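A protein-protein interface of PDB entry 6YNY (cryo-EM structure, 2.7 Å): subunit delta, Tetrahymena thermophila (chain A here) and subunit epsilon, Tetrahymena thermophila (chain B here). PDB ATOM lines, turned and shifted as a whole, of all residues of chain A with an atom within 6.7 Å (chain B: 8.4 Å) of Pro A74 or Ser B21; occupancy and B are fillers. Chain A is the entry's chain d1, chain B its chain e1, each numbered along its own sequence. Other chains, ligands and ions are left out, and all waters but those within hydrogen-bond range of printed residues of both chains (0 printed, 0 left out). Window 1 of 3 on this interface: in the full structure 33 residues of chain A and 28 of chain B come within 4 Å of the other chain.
OG1 of Thr A148 lies within hydrogen-bond range of O of Ser B21 (3.3 Å).
The side-chain hydroxyl (OG) of Ser B21 lies close to the side-chain hydroxyl (OG) of Ser A144 (3.5 Å).
The side-chain hydroxyl of Ser A144 lies within hydrogen-bond range of the side-chain amide oxygen of Asn B17 (3.0 Å).
O of Asn B17 lies within hydrogen-bond range of OG of Ser B21, at 2.7 Å.
The backbone carbonyl oxygen (O) of Thr B59 lies within hydrogen-bond range of a ring nitrogen (NE2) of His B20, 2.4 Å away.
The side-chain carboxylate (OE1) of Glu B23 sits at hydrogen-bond distance from a ring nitrogen (ND1) of His B20, at 3.2 Å.
O of Ala A141 is in hydrogen-bond range of OG of Ser A144.
The backbone carbonyl oxygen (O) of Leu B19 lies within hydrogen-bond range of the side-chain hydroxyl (OG1) of Thr B22, 2.9 Å away.
O of Arg A145 sits at hydrogen-bond distance from OG1 of Thr A148 (2.7 Å).
Leu A72 touches Phe B18.
Thr A95 touches Phe B18 (O to CB, 3.5 Å).
CG2 of Thr B22 touches CG2 of Thr A95, at 3.4 Å.
CG2 of Thr A95 touches CD1 of Leu B29 (3.9 Å).
CE2 of Phe B18 touches C of Gly A96, 3.4 Å away.
Phe B18 touches Gly A97 (CE2 to N, 3.6 Å).
Ala A141 touches His B20 (CB to ND1, 3.4 Å).
Arg A145 touches His B20.
CD of Arg A145 touches N of Gly B24, at 3.4 Å.
CD2 of Phe A152 touches CG1 of Val B25 (3.6 Å).
Of chain B, only Ser B21 comes within 4 Å of Pro A74.
Printed residues of chain A within 4 Å of Ser B21: Pro A74, Ser A144 and Thr A148.
No residue of chain B comes within 4 Å of Gly A75.
Of the printed residues of chain B, Gly A96 touches Phe B18.
Printed residues of chain A within 4 Å of Gly B24: Arg A145.
Printed residues of chain B within 4 Å of Thr A95: Phe B18 (3.5 Å), Thr B22 (3.4 Å) and Leu B29 (3.9 Å).
Printed residues of chain A within 4 Å of Thr B22: Thr A95.
Arg B16 touches none of the printed residues of chain A.
Val A149 touches none of the printed residues of chain B.
The nearest residue of chain B that does not touch Pro A74 is Phe B18 (4.2 Å).
The nearest residue of chain A that does not touch Ser B21 is Arg A145 (4.1 Å).
The nearest printed residue of chain B that does not touch Phe A152 is Leu B29 (4.5 Å).
Of the 18 printed residues of chain B, 8 touch a printed residue of chain A.
Of the 20 printed residues of chain A, 10 touch a printed residue of chain B.
Printed residues of chain A that touch a printed residue of chain B: Leu A72, Pro A74, Thr A95, Gly A96, Gly A97, Ala A141, Ser A144, Arg A145, Thr A148 and Phe A152.
Along chain A the printed residues that touch a printed residue of chain B span positions 72 to 152.
Among the printed residues, no Asp or Glu carboxylate lies within 4 Å of a Lys or Arg side-chain nitrogen of the other chain.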
ATOM      1  N   LYS A  53       3.583 -17.586 -27.633  1.00  0.00           N
ATOM      2  CA  LYS A  53       3.331 -16.929 -26.358  1.00  0.00           C
ATOM      3  C   LYS A  53       2.991 -15.470 -26.616  1.00  0.00           C
ATOM      4  O   LYS A  53       3.824 -14.716 -27.131  1.00  0.00           O
ATOM      5  CB  LYS A  53       4.541 -17.042 -25.425  1.00  0.00           C
ATOM      6  CG  LYS A  53       4.608 -18.346 -24.640  1.00  0.00           C
ATOM      7  CD  LYS A  53       4.886 -19.545 -25.532  1.00  0.00           C
ATOM      8  CE  LYS A  53       4.956 -20.835 -24.730  1.00  0.00           C
ATOM      9  NZ  LYS A  53       6.008 -20.793 -23.679  1.00  0.00           N
ATOM     10  N   LEU A  72       2.753 -10.880 -30.986  1.00  0.00           N
ATOM     11  CA  LEU A  72       3.602 -11.748 -30.192  1.00  0.00           C
ATOM     12  C   LEU A  72       4.826 -10.980 -29.724  1.00  0.00           C
ATOM     13  O   LEU A  72       5.564 -10.450 -30.568  1.00  0.00           O
ATOM     14  CB  LEU A  72       4.029 -12.962 -31.004  1.00  0.00           C
ATOM     15  CG  LEU A  72       2.913 -13.662 -31.778  1.00  0.00           C
ATOM     16  CD1 LEU A  72       3.442 -14.930 -32.420  1.00  0.00           C
ATOM     17  CD2 LEU A  72       1.724 -13.956 -30.881  1.00  0.00           C
ATOM     18  N   PRO A  73       5.088 -10.886 -28.423  1.00  0.00           N
ATOM     19  CA  PRO A  73       6.339 -10.286 -27.969  1.00  0.00           C
ATOM     20  C   PRO A  73       7.518 -11.155 -28.362  1.00  0.00           C
ATOM     21  O   PRO A  73       7.335 -12.239 -28.937  1.00  0.00           O
ATOM     22  CB  PRO A  73       6.171 -10.222 -26.444  1.00  0.00           C
ATOM     23  CG  PRO A  73       5.178 -11.263 -26.128  1.00  0.00           C
ATOM     24  CD  PRO A  73       4.243 -11.308 -27.295  1.00  0.00           C
ATOM     25  N   PRO A  74       8.741 -10.726 -28.067  1.00  0.00           N
ATOM     26  CA  PRO A  74       9.905 -11.544 -28.433  1.00  0.00           C
ATOM     27  C   PRO A  74       9.989 -12.830 -27.628  1.00  0.00           C
ATOM     28  O   PRO A  74      10.802 -12.950 -26.706  1.00  0.00           O
ATOM     29  CB  PRO A  74      11.091 -10.612 -28.146  1.00  0.00           C
ATOM     30  CG  PRO A  74      10.565  -9.613 -27.179  1.00  0.00           C
ATOM     31  CD  PRO A  74       9.138  -9.409 -27.547  1.00  0.00           C
ATOM     32  N   GLY A  75       9.139 -13.796 -27.970  1.00  0.00           N
ATOM     33  CA  GLY A  75       9.130 -15.081 -27.315  1.00  0.00           C
ATOM     34  C   GLY A  75       9.426 -16.212 -28.278  1.00  0.00           C
ATOM     35  O   GLY A  75       9.846 -15.992 -29.419  1.00  0.00           O
ATOM     36  N   PRO A  76       9.211 -17.449 -27.839  1.00  0.00           N
ATOM     37  CA  PRO A  76       9.465 -18.604 -28.702  1.00  0.00           C
ATOM     38  C   PRO A  76       8.281 -18.945 -29.590  1.00  0.00           C
ATOM     39  O   PRO A  76       7.120 -18.691 -29.263  1.00  0.00           O
ATOM     40  CB  PRO A  76       9.733 -19.727 -27.691  1.00  0.00           C
ATOM     41  CG  PRO A  76       8.879 -19.369 -26.527  1.00  0.00           C
ATOM     42  CD  PRO A  76       8.828 -17.859 -26.476  1.00  0.00           C
ATOM     43  N   LEU A  93      13.130 -18.487 -31.869  1.00  0.00           N
ATOM     44  CA  LEU A  93      12.927 -17.360 -30.962  1.00  0.00           C
ATOM     45  C   LEU A  93      12.857 -16.091 -31.799  1.00  0.00           C
ATOM     46  O   LEU A  93      13.852 -15.694 -32.414  1.00  0.00           O
ATOM     47  CB  LEU A  93      14.051 -17.272 -29.931  1.00  0.00           C
ATOM     48  CG  LEU A  93      13.918 -18.132 -28.673  1.00  0.00           C
ATOM     49  CD1 LEU A  93      12.848 -17.564 -27.754  1.00  0.00           C
ATOM     50  CD2 LEU A  93      13.604 -19.571 -29.038  1.00  0.00           C
ATOM     51  N   HIS A  94      11.689 -15.459 -31.825  1.00  0.00           N
ATOM     52  CA  HIS A  94      11.476 -14.253 -32.609  1.00  0.00           C
ATOM     53  C   HIS A  94      11.675 -13.022 -31.734  1.00  0.00           C
ATOM     54  O   HIS A  94      11.498 -13.068 -30.514  1.00  0.00           O
ATOM     55  CB  HIS A  94      10.074 -14.237 -33.218  1.00  0.00           C
ATOM     56  CG  HIS A  94       8.975 -14.278 -32.205  1.00  0.00           C
ATOM     57  ND1 HIS A  94       8.331 -15.444 -31.851  1.00  0.00           N
ATOM     58  CD2 HIS A  94       8.409 -13.297 -31.463  1.00  0.00           C
ATOM     59  CE1 HIS A  94       7.414 -15.178 -30.938  1.00  0.00           C
ATOM     60  NE2 HIS A  94       7.441 -13.883 -30.685  1.00  0.00           N
ATOM     61  N   THR A  95      12.054 -11.919 -32.372  1.00  0.00           N
ATOM     62  CA  THR A  95      12.272 -10.654 -31.682  1.00  0.00           C
ATOM     63  C   THR A  95      11.010  -9.811 -31.577  1.00  0.00           C
ATOM     64  O   THR A  95      11.058  -8.721 -30.999  1.00  0.00           O
ATOM     65  CB  THR A  95      13.360  -9.850 -32.397  1.00  0.00           C
ATOM     66  OG1 THR A  95      13.018  -9.704 -33.781  1.00  0.00           O
ATOM     67  CG2 THR A  95      14.705 -10.547 -32.277  1.00  0.00           C
ATOM     68  N   GLY A  96       9.890 -10.286 -32.115  1.00  0.00           N
ATOM     69  CA  GLY A  96       8.651  -9.536 -32.090  1.00  0.00           C
ATOM     70  C   GLY A  96       7.996  -9.529 -33.453  1.00  0.00           C
ATOM     71  O   GLY A  96       8.677  -9.363 -34.469  1.00  0.00           O
ATOM     72  N   GLY A  97       6.682  -9.713 -33.500  1.00  0.00           N
ATOM     73  CA  GLY A  97       6.006  -9.764 -34.782  1.00  0.00           C
ATOM     74  C   GLY A  97       4.509  -9.638 -34.626  1.00  0.00           C
ATOM     75  O   GLY A  97       3.969  -9.633 -33.516  1.00  0.00           O
ATOM     76  N   ALA A 141      10.704   0.609 -21.088  1.00  0.00           N
ATOM     77  CA  ALA A 141      11.720   0.085 -21.994  1.00  0.00           C
ATOM     78  C   ALA A 141      12.548  -0.997 -21.315  1.00  0.00           C
ATOM     79  O   ALA A 141      12.696  -2.107 -21.839  1.00  0.00           O
ATOM     80  CB  ALA A 141      12.615   1.221 -22.486  1.00  0.00           C
ATOM     81  N   SER A 144      10.566  -4.327 -20.564  1.00  0.00           N
ATOM     82  CA  SER A 144      10.523  -5.324 -21.628  1.00  0.00           C
ATOM     83  C   SER A 144      11.863  -6.035 -21.761  1.00  0.00           C
ATOM     84  O   SER A 144      11.917  -7.265 -21.874  1.00  0.00           O
ATOM     85  CB  SER A 144      10.136  -4.660 -22.948  1.00  0.00           C
ATOM     86  OG  SER A 144      11.056  -3.638 -23.286  1.00  0.00           O
ATOM     87  N   ARG A 145      12.959  -5.273 -21.751  1.00  0.00           N
ATOM     88  CA  ARG A 145      14.279  -5.875 -21.899  1.00  0.00           C
ATOM     89  C   ARG A 145      14.530  -6.923 -20.824  1.00  0.00           C
ATOM     90  O   ARG A 145      15.053  -8.007 -21.111  1.00  0.00           O
ATOM     91  CB  ARG A 145      15.351  -4.789 -21.844  1.00  0.00           C
ATOM     92  CG  ARG A 145      16.770  -5.323 -21.836  1.00  0.00           C
ATOM     93  CD  ARG A 145      17.764  -4.259 -22.256  1.00  0.00           C
ATOM     94  NE  ARG A 145      17.584  -3.022 -21.500  1.00  0.00           N
ATOM     95  CZ  ARG A 145      18.092  -2.800 -20.292  1.00  0.00           C
ATOM     96  NH1 ARG A 145      17.874  -1.641 -19.686  1.00  0.00           N
ATOM     97  NH2 ARG A 145      18.810  -3.735 -19.683  1.00  0.00           N
ATOM     98  N   LYS A 146      14.159  -6.621 -19.579  1.00  0.00           N
ATOM     99  CA  LYS A 146      14.325  -7.591 -18.502  1.00  0.00           C
ATOM    100  C   LYS A 146      13.453  -8.817 -18.732  1.00  0.00           C
ATOM    101  O   LYS A 146      13.874  -9.949 -18.467  1.00  0.00           O
ATOM    102  CB  LYS A 146      13.988  -6.938 -17.165  1.00  0.00           C
ATOM    103  CG  LYS A 146      14.921  -5.802 -16.782  1.00  0.00           C
ATOM    104  CD  LYS A 146      14.554  -5.196 -15.437  1.00  0.00           C
ATOM    105  CE  LYS A 146      13.185  -4.531 -15.474  1.00  0.00           C
ATOM    106  NZ  LYS A 146      12.857  -3.859 -14.188  1.00  0.00           N
ATOM    107  N   SER A 147      12.231  -8.609 -19.225  1.00  0.00           N
ATOM    108  CA  SER A 147      11.321  -9.728 -19.448  1.00  0.00           C
ATOM    109  C   SER A 147      11.902 -10.716 -20.450  1.00  0.00           C
ATOM    110  O   SER A 147      11.817 -11.934 -20.254  1.00  0.00           O
ATOM    111  CB  SER A 147       9.967  -9.210 -19.927  1.00  0.00           C
ATOM    112  OG  SER A 147       9.059 -10.278 -20.138  1.00  0.00           O
ATOM    113  N   THR A 148      12.499 -10.210 -21.531  1.00  0.00           N
ATOM    114  CA  THR A 148      13.073 -11.098 -22.535  1.00  0.00           C
ATOM    115  C   THR A 148      14.242 -11.890 -21.968  1.00  0.00           C
ATOM    116  O   THR A 148      14.378 -13.088 -22.243  1.00  0.00           O
ATOM    117  CB  THR A 148      13.527 -10.291 -23.749  1.00  0.00           C
ATOM    118  OG1 THR A 148      14.589  -9.408 -23.367  1.00  0.00           O
ATOM    119  CG2 THR A 148      12.377  -9.478 -24.303  1.00  0.00           C
ATOM    120  N   VAL A 149      15.101 -11.239 -21.182  1.00  0.00           N
ATOM    121  CA  VAL A 149      16.226 -11.943 -20.574  1.00  0.00           C
ATOM    122  C   VAL A 149      15.722 -13.121 -19.751  1.00  0.00           C
ATOM    123  O   VAL A 149      16.233 -14.243 -19.859  1.00  0.00           O
ATOM    124  CB  VAL A 149      17.063 -10.975 -19.719  1.00  0.00           C
ATOM    125  CG1 VAL A 149      18.117 -11.737 -18.931  1.00  0.00           C
ATOM    126  CG2 VAL A 149      17.709  -9.913 -20.602  1.00  0.00           C
ATOM    127  N   LEU A 151      12.884 -14.579 -20.136  1.00  0.00           N
ATOM    128  CA  LEU A 151      12.267 -15.510 -21.073  1.00  0.00           C
ATOM    129  C   LEU A 151      13.321 -16.321 -21.815  1.00  0.00           C
ATOM    130  O   LEU A 151      13.251 -17.555 -21.864  1.00  0.00           O
ATOM    131  CB  LEU A 151      11.384 -14.744 -22.059  1.00  0.00           C
ATOM    132  CG  LEU A 151      10.645 -15.578 -23.109  1.00  0.00           C
ATOM    133  CD1 LEU A 151       9.311 -14.939 -23.439  1.00  0.00           C
ATOM    134  CD2 LEU A 151      11.471 -15.735 -24.375  1.00  0.00           C
ATOM    135  N   PHE A 152      14.307 -15.640 -22.404  1.00  0.00           N
ATOM    136  CA  PHE A 152      15.319 -16.331 -23.196  1.00  0.00           C
ATOM    137  C   PHE A 152      16.052 -17.379 -22.370  1.00  0.00           C
ATOM    138  O   PHE A 152      16.301 -18.493 -22.849  1.00  0.00           O
ATOM    139  CB  PHE A 152      16.309 -15.320 -23.773  1.00  0.00           C
ATOM    140  CG  PHE A 152      15.780 -14.548 -24.952  1.00  0.00           C
ATOM    141  CD1 PHE A 152      14.423 -14.489 -25.215  1.00  0.00           C
ATOM    142  CD2 PHE A 152      16.648 -13.889 -25.803  1.00  0.00           C
ATOM    143  CE1 PHE A 152      13.942 -13.782 -26.298  1.00  0.00           C
ATOM    144  CE2 PHE A 152      16.173 -13.180 -26.889  1.00  0.00           C
ATOM    145  CZ  PHE A 152      14.819 -13.127 -27.137  1.00  0.00           C
ATOM    146  N   CYS B   2       6.078  -5.312 -20.382  1.00  0.00           N
ATOM    147  CA  CYS B   2       4.736  -5.256 -20.949  1.00  0.00           C
ATOM    148  C   CYS B   2       4.732  -4.453 -22.241  1.00  0.00           C
ATOM    149  O   CYS B   2       5.464  -3.473 -22.375  1.00  0.00           O
ATOM    150  CB  CYS B   2       3.758  -4.643 -19.949  1.00  0.00           C
ATOM    151  SG  CYS B   2       4.132  -2.934 -19.515  1.00  0.00           S
ATOM    152  N   ILE B   3       3.898  -4.871 -23.192  1.00  0.00           N
ATOM    153  CA  ILE B   3       3.811  -4.202 -24.484  1.00  0.00           C
ATOM    154  C   ILE B   3       2.621  -3.252 -24.502  1.00  0.00           C
ATOM    155  O   ILE B   3       2.643  -2.226 -25.192  1.00  0.00           O
ATOM    156  CB  ILE B   3       3.712  -5.230 -25.627  1.00  0.00           C
ATOM    157  CG1 ILE B   3       2.386  -5.986 -25.564  1.00  0.00           C
ATOM    158  CG2 ILE B   3       4.863  -6.214 -25.547  1.00  0.00           C
ATOM    159  CD1 ILE B   3       2.239  -7.034 -26.639  1.00  0.00           C
ATOM    160  N   ILE B  14       5.314  -0.065 -30.927  1.00  0.00           N
ATOM    161  CA  ILE B  14       5.622  -1.488 -30.810  1.00  0.00           C
ATOM    162  C   ILE B  14       7.030  -1.775 -31.311  1.00  0.00           C
ATOM    163  O   ILE B  14       7.781  -2.538 -30.693  1.00  0.00           O
ATOM    164  CB  ILE B  14       4.575  -2.321 -31.568  1.00  0.00           C
ATOM    165  CG1 ILE B  14       4.773  -3.808 -31.276  1.00  0.00           C
ATOM    166  CG2 ILE B  14       4.662  -2.058 -33.059  1.00  0.00           C
ATOM    167  CD1 ILE B  14       3.760  -4.696 -31.947  1.00  0.00           C
ATOM    168  N   VAL B  15       7.411  -1.169 -32.436  1.00  0.00           N
ATOM    169  CA  VAL B  15       8.730  -1.430 -33.006  1.00  0.00           C
ATOM    170  C   VAL B  15       9.818  -1.010 -32.028  1.00  0.00           C
ATOM    171  O   VAL B  15      10.762  -1.763 -31.760  1.00  0.00           O
ATOM    172  CB  VAL B  15       8.879  -0.715 -34.360  1.00  0.00           C
ATOM    173  CG1 VAL B  15      10.249  -0.984 -34.949  1.00  0.00           C
ATOM    174  CG2 VAL B  15       7.790  -1.167 -35.314  1.00  0.00           C
ATOM    175  N   ARG B  16       9.701   0.199 -31.475  1.00  0.00           N
ATOM    176  CA  ARG B  16      10.677   0.645 -30.488  1.00  0.00           C
ATOM    177  C   ARG B  16      10.737  -0.325 -29.317  1.00  0.00           C
ATOM    178  O   ARG B  16      11.811  -0.568 -28.754  1.00  0.00           O
ATOM    179  CB  ARG B  16      10.333   2.054 -30.003  1.00  0.00           C
ATOM    180  CG  ARG B  16      11.179   2.520 -28.830  1.00  0.00           C
ATOM    181  CD  ARG B  16      10.917   3.975 -28.492  1.00  0.00           C
ATOM    182  NE  ARG B  16      11.701   4.418 -27.344  1.00  0.00           N
ATOM    183  CZ  ARG B  16      11.719   5.665 -26.888  1.00  0.00           C
ATOM    184  NH1 ARG B  16      10.997   6.607 -27.480  1.00  0.00           N
ATOM    185  NH2 ARG B  16      12.465   5.973 -25.837  1.00  0.00           N
ATOM    186  N   ASN B  17       9.591  -0.893 -28.940  1.00  0.00           N
ATOM    187  CA  ASN B  17       9.569  -1.844 -27.837  1.00  0.00           C
ATOM    188  C   ASN B  17      10.357  -3.098 -28.184  1.00  0.00           C
ATOM    189  O   ASN B  17      11.133  -3.600 -27.362  1.00  0.00           O
ATOM    190  CB  ASN B  17       8.126  -2.196 -27.482  1.00  0.00           C
ATOM    191  CG  ASN B  17       8.019  -2.989 -26.198  1.00  0.00           C
ATOM    192  OD1 ASN B  17       9.008  -3.185 -25.490  1.00  0.00           O
ATOM    193  ND2 ASN B  17       6.815  -3.446 -25.884  1.00  0.00           N
ATOM    194  N   PHE B  18      10.175  -3.619 -29.400  1.00  0.00           N
ATOM    195  CA  PHE B  18      10.965  -4.766 -29.829  1.00  0.00           C
ATOM    196  C   PHE B  18      12.449  -4.432 -29.842  1.00  0.00           C
ATOM    197  O   PHE B  18      13.288  -5.281 -29.514  1.00  0.00           O
ATOM    198  CB  PHE B  18      10.518  -5.224 -31.218  1.00  0.00           C
ATOM    199  CG  PHE B  18       9.110  -5.755 -31.270  1.00  0.00           C
ATOM    200  CD1 PHE B  18       8.464  -6.189 -30.126  1.00  0.00           C
ATOM    201  CD2 PHE B  18       8.435  -5.824 -32.478  1.00  0.00           C
ATOM    202  CE1 PHE B  18       7.175  -6.678 -30.186  1.00  0.00           C
ATOM    203  CE2 PHE B  18       7.147  -6.312 -32.541  1.00  0.00           C
ATOM    204  CZ  PHE B  18       6.517  -6.739 -31.394  1.00  0.00           C
ATOM    205  N   LEU B  19      12.796  -3.199 -30.215  1.00  0.00           N
ATOM    206  CA  LEU B  19      14.199  -2.804 -30.229  1.00  0.00           C
ATOM    207  C   LEU B  19      14.773  -2.780 -28.819  1.00  0.00           C
ATOM    208  O   LEU B  19      15.815  -3.390 -28.551  1.00  0.00           O
ATOM    209  CB  LEU B  19      14.348  -1.437 -30.895  1.00  0.00           C
ATOM    210  CG  LEU B  19      13.956  -1.375 -32.372  1.00  0.00           C
ATOM    211  CD1 LEU B  19      14.021   0.054 -32.884  1.00  0.00           C
ATOM    212  CD2 LEU B  19      14.841  -2.286 -33.204  1.00  0.00           C
ATOM    213  N   HIS B  20      14.106  -2.078 -27.900  1.00  0.00           N
ATOM    214  CA  HIS B  20      14.547  -2.091 -26.511  1.00  0.00           C
ATOM    215  C   HIS B  20      14.569  -3.504 -25.951  1.00  0.00           C
ATOM    216  O   HIS B  20      15.411  -3.825 -25.104  1.00  0.00           O
ATOM    217  CB  HIS B  20      13.640  -1.199 -25.666  1.00  0.00           C
ATOM    218  CG  HIS B  20      13.892   0.263 -25.848  1.00  0.00           C
ATOM    219  ND1 HIS B  20      14.825   0.954 -25.106  1.00  0.00           N
ATOM    220  CD2 HIS B  20      13.333   1.167 -26.686  1.00  0.00           C
ATOM    221  CE1 HIS B  20      14.829   2.221 -25.478  1.00  0.00           C
ATOM    222  NE2 HIS B  20      13.934   2.377 -26.437  1.00  0.00           N
ATOM    223  N   SER B  21      13.654  -4.362 -26.407  1.00  0.00           N
ATOM    224  CA  SER B  21      13.643  -5.745 -25.947  1.00  0.00           C
ATOM    225  C   SER B  21      14.906  -6.472 -26.388  1.00  0.00           C
ATOM    226  O   SER B  21      15.585  -7.114 -25.580  1.00  0.00           O
ATOM    227  CB  SER B  21      12.397  -6.454 -26.473  1.00  0.00           C
ATOM    228  OG  SER B  21      11.220  -5.888 -25.923  1.00  0.00           O
ATOM    229  N   THR B  22      15.239  -6.376 -27.677  1.00  0.00           N
ATOM    230  CA  THR B  22      16.445  -7.011 -28.189  1.00  0.00           C
ATOM    231  C   THR B  22      17.705  -6.296 -27.727  1.00  0.00           C
ATOM    232  O   THR B  22      18.781  -6.903 -27.726  1.00  0.00           O
ATOM    233  CB  THR B  22      16.414  -7.055 -29.718  1.00  0.00           C
ATOM    234  OG1 THR B  22      16.321  -5.722 -30.236  1.00  0.00           O
ATOM    235  CG2 THR B  22      15.230  -7.873 -30.204  1.00  0.00           C
ATOM    236  N   GLU B  23      17.588  -5.023 -27.334  1.00  0.00           N
ATOM    237  CA  GLU B  23      18.753  -4.249 -26.918  1.00  0.00           C
ATOM    238  C   GLU B  23      19.629  -5.037 -25.954  1.00  0.00           C
ATOM    239  O   GLU B  23      20.862  -4.964 -26.018  1.00  0.00           O
ATOM    240  CB  GLU B  23      18.294  -2.939 -26.274  1.00  0.00           C
ATOM    241  CG  GLU B  23      19.420  -2.040 -25.804  1.00  0.00           C
ATOM    242  CD  GLU B  23      18.912  -0.751 -25.188  1.00  0.00           C
ATOM    243  OE1 GLU B  23      17.679  -0.568 -25.120  1.00  0.00           O
ATOM    244  OE2 GLU B  23      19.747   0.080 -24.771  1.00  0.00           O
ATOM    245  N   GLY B  24      19.011  -5.796 -25.051  1.00  0.00           N
ATOM    246  CA  GLY B  24      19.756  -6.573 -24.082  1.00  0.00           C
ATOM    247  C   GLY B  24      20.308  -7.881 -24.600  1.00  0.00           C
ATOM    248  O   GLY B  24      21.124  -8.504 -23.913  1.00  0.00           O
ATOM    249  N   VAL B  25      19.887  -8.314 -25.788  1.00  0.00           N
ATOM    250  CA  VAL B  25      20.285  -9.614 -26.318  1.00  0.00           C
ATOM    251  C   VAL B  25      20.861  -9.483 -27.724  1.00  0.00           C
ATOM    252  O   VAL B  25      21.133 -10.492 -28.384  1.00  0.00           O
ATOM    253  CB  VAL B  25      19.095 -10.592 -26.314  1.00  0.00           C
ATOM    254  CG1 VAL B  25      19.560 -11.992 -26.677  1.00  0.00           C
ATOM    255  CG2 VAL B  25      18.410 -10.589 -24.958  1.00  0.00           C
ATOM    256  N   ILE B  26      21.062  -8.251 -28.196  1.00  0.00           N
ATOM    257  CA  ILE B  26      21.607  -8.073 -29.539  1.00  0.00           C
ATOM    258  C   ILE B  26      22.938  -8.803 -29.671  1.00  0.00           C
ATOM    259  O   ILE B  26      23.233  -9.402 -30.712  1.00  0.00           O
ATOM    260  CB  ILE B  26      21.749  -6.576 -29.877  1.00  0.00           C
ATOM    261  CG1 ILE B  26      22.611  -5.860 -28.834  1.00  0.00           C
ATOM    262  CG2 ILE B  26      20.384  -5.917 -29.983  1.00  0.00           C
ATOM    263  CD1 ILE B  26      22.803  -4.388 -29.119  1.00  0.00           C
ATOM    264  N   LEU B  29      22.382 -12.710 -29.964  1.00  0.00           N
ATOM    265  CA  LEU B  29      21.938 -13.190 -31.260  1.00  0.00           C
ATOM    266  C   LEU B  29      23.105 -13.206 -32.246  1.00  0.00           C
ATOM    267  O   LEU B  29      24.073 -12.456 -32.090  1.00  0.00           O
ATOM    268  CB  LEU B  29      20.814 -12.311 -31.801  1.00  0.00           C
ATOM    269  CG  LEU B  29      19.631 -12.089 -30.858  1.00  0.00           C
ATOM    270  CD1 LEU B  29      18.441 -11.546 -31.630  1.00  0.00           C
ATOM    271  CD2 LEU B  29      19.266 -13.373 -30.129  1.00  0.00           C
ATOM    272  N   LEU B  37      19.528  -5.097 -37.119  1.00  0.00           N
ATOM    273  CA  LEU B  37      19.093  -4.113 -36.128  1.00  0.00           C
ATOM    274  C   LEU B  37      20.044  -2.919 -36.167  1.00  0.00           C
ATOM    275  O   LEU B  37      20.942  -2.764 -35.336  1.00  0.00           O
ATOM    276  CB  LEU B  37      19.039  -4.737 -34.740  1.00  0.00           C
ATOM    277  CG  LEU B  37      18.277  -6.057 -34.627  1.00  0.00           C
ATOM    278  CD1 LEU B  37      18.229  -6.521 -33.180  1.00  0.00           C
ATOM    279  CD2 LEU B  37      16.875  -5.923 -35.195  1.00  0.00           C
ATOM    280  N   THR B  59      16.768   4.246 -30.204  1.00  0.00           N
ATOM    281  CA  THR B  59      16.149   3.637 -29.031  1.00  0.00           C
ATOM    282  C   THR B  59      15.544   4.658 -28.085  1.00  0.00           C
ATOM    283  O   THR B  59      14.450   4.437 -27.560  1.00  0.00           O
ATOM    284  CB  THR B  59      17.177   2.795 -28.267  1.00  0.00           C
ATOM    285  OG1 THR B  59      18.295   3.612 -27.903  1.00  0.00           O
ATOM    286  CG2 THR B  59      17.654   1.633 -29.123  1.00  0.00           C
